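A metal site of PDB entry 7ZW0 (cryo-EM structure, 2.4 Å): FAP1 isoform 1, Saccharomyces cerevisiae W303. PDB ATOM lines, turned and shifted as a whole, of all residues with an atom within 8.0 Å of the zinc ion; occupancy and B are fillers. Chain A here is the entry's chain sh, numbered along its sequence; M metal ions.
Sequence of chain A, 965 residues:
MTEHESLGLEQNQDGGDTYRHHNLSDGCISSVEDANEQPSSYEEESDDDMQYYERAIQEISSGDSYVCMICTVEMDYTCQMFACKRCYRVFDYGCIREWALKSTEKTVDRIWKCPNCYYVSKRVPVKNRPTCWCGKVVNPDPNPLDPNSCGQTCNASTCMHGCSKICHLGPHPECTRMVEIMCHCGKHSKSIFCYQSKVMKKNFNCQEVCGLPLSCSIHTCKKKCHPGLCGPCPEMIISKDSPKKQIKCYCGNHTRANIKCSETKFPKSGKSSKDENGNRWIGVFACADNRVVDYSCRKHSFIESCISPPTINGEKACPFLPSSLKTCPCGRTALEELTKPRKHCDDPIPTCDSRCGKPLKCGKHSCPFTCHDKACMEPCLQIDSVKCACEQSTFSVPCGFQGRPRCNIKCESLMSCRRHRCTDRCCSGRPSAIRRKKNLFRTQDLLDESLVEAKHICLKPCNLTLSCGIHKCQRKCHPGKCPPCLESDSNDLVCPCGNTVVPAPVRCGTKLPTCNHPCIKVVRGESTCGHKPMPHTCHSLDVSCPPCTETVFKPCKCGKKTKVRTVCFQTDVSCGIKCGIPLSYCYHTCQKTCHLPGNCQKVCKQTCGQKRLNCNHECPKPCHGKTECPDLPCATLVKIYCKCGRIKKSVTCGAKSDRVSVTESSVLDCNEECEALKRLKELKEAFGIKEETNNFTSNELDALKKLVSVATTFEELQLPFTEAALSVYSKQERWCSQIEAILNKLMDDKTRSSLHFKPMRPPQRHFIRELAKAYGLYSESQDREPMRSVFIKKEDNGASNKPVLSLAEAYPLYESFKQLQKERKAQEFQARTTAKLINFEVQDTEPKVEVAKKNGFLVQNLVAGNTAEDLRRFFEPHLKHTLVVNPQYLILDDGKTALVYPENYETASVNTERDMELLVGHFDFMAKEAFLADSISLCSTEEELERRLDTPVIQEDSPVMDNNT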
ATOM      1  N   TYR A 641      -3.214  13.251  27.787  1.00  0.00           N
ATOM      2  CA  TYR A 641      -2.962  14.119  26.638  1.00  0.00           C
ATOM      3  C   TYR A 641      -4.047  15.128  26.374  1.00  0.00           C
ATOM      4  O   TYR A 641      -5.230  14.799  26.459  1.00  0.00           O
ATOM      5  CB  TYR A 641      -2.766  13.294  25.368  1.00  0.00           C
ATOM      6  CG  TYR A 641      -1.356  12.821  25.126  1.00  0.00           C
ATOM      7  CD1 TYR A 641      -0.469  13.605  24.388  1.00  0.00           C
ATOM      8  CD2 TYR A 641      -0.917  11.603  25.599  1.00  0.00           C
ATOM      9  CE1 TYR A 641       0.818  13.167  24.147  1.00  0.00           C
ATOM     10  CE2 TYR A 641       0.370  11.165  25.358  1.00  0.00           C
ATOM     11  CZ  TYR A 641       1.231  11.950  24.640  1.00  0.00           C
ATOM     12  OH  TYR A 641       2.518  11.512  24.398  1.00  0.00           O
ATOM     13  N   CYS A 642      -3.683  16.346  25.990  1.00  0.00           N
ATOM     14  CA  CYS A 642      -4.683  17.360  25.636  1.00  0.00           C
ATOM     15  C   CYS A 642      -5.373  17.007  24.327  1.00  0.00           C
ATOM     16  O   CYS A 642      -5.025  16.022  23.669  1.00  0.00           O
ATOM     17  CB  CYS A 642      -4.065  18.750  25.578  1.00  0.00           C
ATOM     18  SG  CYS A 642      -2.710  18.925  24.389  1.00  0.00           S
ATOM     19  N   LYS A 643      -6.352  17.818  23.917  1.00  0.00           N
ATOM     20  CA  LYS A 643      -7.109  17.479  22.712  1.00  0.00           C
ATOM     21  C   LYS A 643      -6.242  17.430  21.459  1.00  0.00           C
ATOM     22  O   LYS A 643      -6.399  16.532  20.636  1.00  0.00           O
ATOM     23  CB  LYS A 643      -8.277  18.449  22.520  1.00  0.00           C
ATOM     24  CG  LYS A 643      -9.658  17.810  22.636  1.00  0.00           C
ATOM     25  CD  LYS A 643      -9.815  17.087  23.961  1.00  0.00           C
ATOM     26  CE  LYS A 643     -11.217  16.557  24.164  1.00  0.00           C
ATOM     27  NZ  LYS A 643     -11.358  15.918  25.501  1.00  0.00           N
ATOM     28  N   CYS A 644      -5.335  18.388  21.307  1.00  0.00           N
ATOM     29  CA  CYS A 644      -4.428  18.367  20.165  1.00  0.00           C
ATOM     30  C   CYS A 644      -3.224  17.458  20.377  1.00  0.00           C
ATOM     31  O   CYS A 644      -2.487  17.167  19.443  1.00  0.00           O
ATOM     32  CB  CYS A 644      -3.979  19.784  19.783  1.00  0.00           C
ATOM     33  SG  CYS A 644      -2.993  20.618  21.044  1.00  0.00           S
ATOM     34  N   GLY A 645      -3.014  17.013  21.618  1.00  0.00           N
ATOM     35  CA  GLY A 645      -1.914  16.100  21.907  1.00  0.00           C
ATOM     36  C   GLY A 645      -0.551  16.758  22.068  1.00  0.00           C
ATOM     37  O   GLY A 645       0.467  16.059  22.116  1.00  0.00           O
ATOM     38  N   ARG A 646      -0.513  18.078  22.140  1.00  0.00           N
ATOM     39  CA  ARG A 646       0.754  18.792  22.286  1.00  0.00           C
ATOM     40  C   ARG A 646       1.365  18.563  23.667  1.00  0.00           C
ATOM     41  O   ARG A 646       2.335  17.819  23.797  1.00  0.00           O
ATOM     42  CB  ARG A 646       0.543  20.294  22.058  1.00  0.00           C
ATOM     43  CG  ARG A 646       1.824  21.120  22.066  1.00  0.00           C
ATOM     44  CD  ARG A 646       2.752  20.717  20.936  1.00  0.00           C
ATOM     45  NE  ARG A 646       3.925  21.587  20.861  1.00  0.00           N
ATOM     46  CZ  ARG A 646       4.006  22.670  20.092  1.00  0.00           C
ATOM     47  NH1 ARG A 646       2.991  23.017  19.325  1.00  0.00           N
ATOM     48  NH2 ARG A 646       5.114  23.401  20.097  1.00  0.00           N
ATOM     49  N   ILE A 647       0.801  19.187  24.701  1.00  0.00           N
ATOM     50  CA  ILE A 647       1.318  19.025  26.058  1.00  0.00           C
ATOM     51  C   ILE A 647       0.704  17.856  26.805  1.00  0.00           C
ATOM     52  O   ILE A 647      -0.472  17.549  26.638  1.00  0.00           O
ATOM     53  CB  ILE A 647       1.171  20.318  26.888  1.00  0.00           C
ATOM     54  CG1 ILE A 647       0.157  21.266  26.243  1.00  0.00           C
ATOM     55  CG2 ILE A 647       2.523  21.022  27.014  1.00  0.00           C
ATOM     56  CD1 ILE A 647       0.272  22.692  26.735  1.00  0.00           C
ATOM     57  N   LYS A 648       1.505  17.208  27.641  1.00  0.00           N
ATOM     58  CA  LYS A 648       1.025  16.029  28.374  1.00  0.00           C
ATOM     59  C   LYS A 648       1.352  16.148  29.862  1.00  0.00           C
ATOM     60  O   LYS A 648       2.371  16.724  30.237  1.00  0.00           O
ATOM     61  CB  LYS A 648       1.670  14.783  27.774  1.00  0.00           C
ATOM     62  CG  LYS A 648       3.112  15.003  27.356  1.00  0.00           C
ATOM     63  CD  LYS A 648       3.630  13.865  26.505  1.00  0.00           C
ATOM     64  CE  LYS A 648       5.068  14.105  26.076  1.00  0.00           C
ATOM     65  NZ  LYS A 648       5.593  12.974  25.267  1.00  0.00           N
ATOM     66  N   LEU A 668      -7.421  15.093  28.373  1.00  0.00           N
ATOM     67  CA  LEU A 668      -7.435  16.507  28.736  1.00  0.00           C
ATOM     68  C   LEU A 668      -8.048  17.375  27.661  1.00  0.00           C
ATOM     69  O   LEU A 668      -7.856  17.124  26.483  1.00  0.00           O
ATOM     70  CB  LEU A 668      -6.025  16.990  29.028  1.00  0.00           C
ATOM     71  CG  LEU A 668      -5.276  16.442  30.227  1.00  0.00           C
ATOM     72  CD1 LEU A 668      -3.815  16.833  30.133  1.00  0.00           C
ATOM     73  CD2 LEU A 668      -5.888  16.972  31.513  1.00  0.00           C
ATOM     74  N   ASP A 669      -8.801  18.383  28.074  1.00  0.00           N
ATOM     75  CA  ASP A 669      -9.326  19.331  27.101  1.00  0.00           C
ATOM     76  C   ASP A 669      -8.151  20.216  26.710  1.00  0.00           C
ATOM     77  O   ASP A 669      -7.190  20.314  27.469  1.00  0.00           O
ATOM     78  CB  ASP A 669     -10.440  20.173  27.715  1.00  0.00           C
ATOM     79  CG  ASP A 669     -11.626  19.333  28.166  1.00  0.00           C
ATOM     80  OD1 ASP A 669     -11.634  18.116  27.904  1.00  0.00           O
ATOM     81  OD2 ASP A 669     -12.554  19.904  28.780  1.00  0.00           O
ATOM     82  N   CYS A 670      -8.208  20.853  25.547  1.00  0.00           N
ATOM     83  CA  CYS A 670      -7.139  21.782  25.182  1.00  0.00           C
ATOM     84  C   CYS A 670      -7.071  22.904  26.222  1.00  0.00           C
ATOM     85  O   CYS A 670      -8.072  23.583  26.466  1.00  0.00           O
ATOM     86  CB  CYS A 670      -7.391  22.381  23.798  1.00  0.00           C
ATOM     87  SG  CYS A 670      -6.463  21.598  22.463  1.00  0.00           S
ATOM     88  N   ASN A 671      -5.907  23.085  26.836  1.00  0.00           N
ATOM     89  CA  ASN A 671      -5.768  24.115  27.858  1.00  0.00           C
ATOM     90  C   ASN A 671      -5.728  25.472  27.180  1.00  0.00           C
ATOM     91  O   ASN A 671      -5.650  25.540  25.960  1.00  0.00           O
ATOM     92  CB  ASN A 671      -4.545  23.890  28.749  1.00  0.00           C
ATOM     93  CG  ASN A 671      -3.236  24.000  27.994  1.00  0.00           C
ATOM     94  OD1 ASN A 671      -3.020  23.298  27.006  1.00  0.00           O
ATOM     95  ND2 ASN A 671      -2.350  24.858  28.476  1.00  0.00           N
ATOM     96  N   GLU A 672      -5.788  26.546  27.945  1.00  0.00           N
ATOM     97  CA  GLU A 672      -5.848  27.868  27.342  1.00  0.00           C
ATOM     98  C   GLU A 672      -4.642  28.164  26.472  1.00  0.00           C
ATOM     99  O   GLU A 672      -4.777  28.802  25.439  1.00  0.00           O
ATOM    100  CB  GLU A 672      -6.006  28.962  28.406  1.00  0.00           C
ATOM    101  CG  GLU A 672      -7.372  28.961  29.072  1.00  0.00           C
ATOM    102  CD  GLU A 672      -7.595  30.193  29.942  1.00  0.00           C
ATOM    103  OE1 GLU A 672      -8.684  30.303  30.547  1.00  0.00           O
ATOM    104  OE2 GLU A 672      -6.683  31.044  30.011  1.00  0.00           O
ATOM    105  N   GLU A 673      -3.452  27.726  26.882  1.00  0.00           N
ATOM    106  CA  GLU A 673      -2.275  27.913  26.035  1.00  0.00           C
ATOM    107  C   GLU A 673      -2.419  27.147  24.721  1.00  0.00           C
ATOM    108  O   GLU A 673      -2.083  27.666  23.661  1.00  0.00           O
ATOM    109  CB  GLU A 673      -1.004  27.463  26.753  1.00  0.00           C
ATOM    110  CG  GLU A 673      -0.688  28.252  28.010  1.00  0.00           C
ATOM    111  CD  GLU A 673       0.603  27.794  28.668  1.00  0.00           C
ATOM    112  OE1 GLU A 673       1.009  28.411  29.669  1.00  0.00           O
ATOM    113  OE2 GLU A 673       1.201  26.811  28.177  1.00  0.00           O
ATOM    114  N   CYS A 674      -2.920  25.916  24.782  1.00  0.00           N
ATOM    115  CA  CYS A 674      -3.159  25.161  23.541  1.00  0.00           C
ATOM    116  C   CYS A 674      -4.256  25.829  22.740  1.00  0.00           C
ATOM    117  O   CYS A 674      -4.195  25.857  21.515  1.00  0.00           O
ATOM    118  CB  CYS A 674      -3.526  23.714  23.826  1.00  0.00           C
ATOM    119  SG  CYS A 674      -2.111  22.603  23.838  1.00  0.00           S
ATOM    120  N   GLU A 675      -5.263  26.363  23.418  1.00  0.00           N
ATOM    121  CA  GLU A 675      -6.320  27.081  22.732  1.00  0.00           C
ATOM    122  C   GLU A 675      -5.778  28.326  22.071  1.00  0.00           C
ATOM    123  O   GLU A 675      -6.189  28.656  20.973  1.00  0.00           O
ATOM    124  CB  GLU A 675      -7.451  27.437  23.696  1.00  0.00           C
ATOM    125  CG  GLU A 675      -8.427  26.296  23.942  1.00  0.00           C
ATOM    126  CD  GLU A 675      -9.270  25.983  22.711  1.00  0.00           C
ATOM    127  OE1 GLU A 675      -9.674  24.805  22.556  1.00  0.00           O
ATOM    128  OE2 GLU A 675      -9.528  26.897  21.908  1.00  0.00           O
ATOM    129  N   LEU A 677      -2.724  28.749  20.981  1.00  0.00           N
ATOM    130  CA  LEU A 677      -1.990  28.282  19.816  1.00  0.00           C
ATOM    131  C   LEU A 677      -2.962  27.885  18.717  1.00  0.00           C
ATOM    132  O   LEU A 677      -2.726  28.154  17.543  1.00  0.00           O
ATOM    133  CB  LEU A 677      -1.098  27.105  20.195  1.00  0.00           C
ATOM    134  CG  LEU A 677       0.363  27.213  19.770  1.00  0.00           C
ATOM    135  CD1 LEU A 677       1.164  26.032  20.282  1.00  0.00           C
ATOM    136  CD2 LEU A 677       0.449  27.332  18.255  1.00  0.00           C
ATOM    137  N   LYS A 678      -4.055  27.241  19.103  1.00  0.00           N
ATOM    138  CA  LYS A 678      -5.080  26.867  18.141  1.00  0.00           C
ATOM    139  C   LYS A 678      -5.651  28.137  17.536  1.00  0.00           C
ATOM    140  O   LYS A 678      -5.902  28.188  16.348  1.00  0.00           O
ATOM    141  CB  LYS A 678      -6.176  26.067  18.831  1.00  0.00           C
ATOM    142  CG  LYS A 678      -7.326  25.635  17.937  1.00  0.00           C
ATOM    143  CD  LYS A 678      -8.429  24.998  18.768  1.00  0.00           C
ATOM    144  CE  LYS A 678      -9.594  24.563  17.899  1.00  0.00           C
ATOM    145  NZ  LYS A 678     -10.718  24.002  18.706  1.00  0.00           N
HETATM  146 ZN    ZN M   1      -3.781  20.918  23.085  1.00  0.00          ZN
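Of the 18 residues printed, 4 come within 4 Å of the zinc ion. The nearest printed residue that does not touch the zinc ion is Lys 643 (4.1 Å).
The backbone carbonyl oxygen (O) of Ile 647 is in hydrogen-bond range of the backbone NH (N) of Cys 642, 3.5 Å away. SG of Cys 644 sits close to N of Arg 646 (3.7 Å). The backbone NH (N) of Cys 644 is in hydrogen-bond range of the side-chain sulfur (SG) of Cys 670 (3.6 Å). The backbone NH (N) of Gly 645 lies close to the side-chain sulfur (SG) of Cys 642, at 3.4 Å. N of Cys 674 sits close to OD1 of Asn 671 (3.4 Å). The backbone NH (N) of Arg 646 lies close to the side-chain sulfur (SG) of Cys 642 (3.3 Å).
The zinc ion is bound by SG of Cys 644. The zinc ion is bound by the side-chain sulfur (SG) of Cys 674 (2.5 Å). The zinc ion is bound by the side-chain sulfur (SG) of Cys 642, at 2.6 Å. The zinc ion has three donor atoms within binding distance. Slightly farther from the zinc ion lies SG of Cys 670 (2.8 Å).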
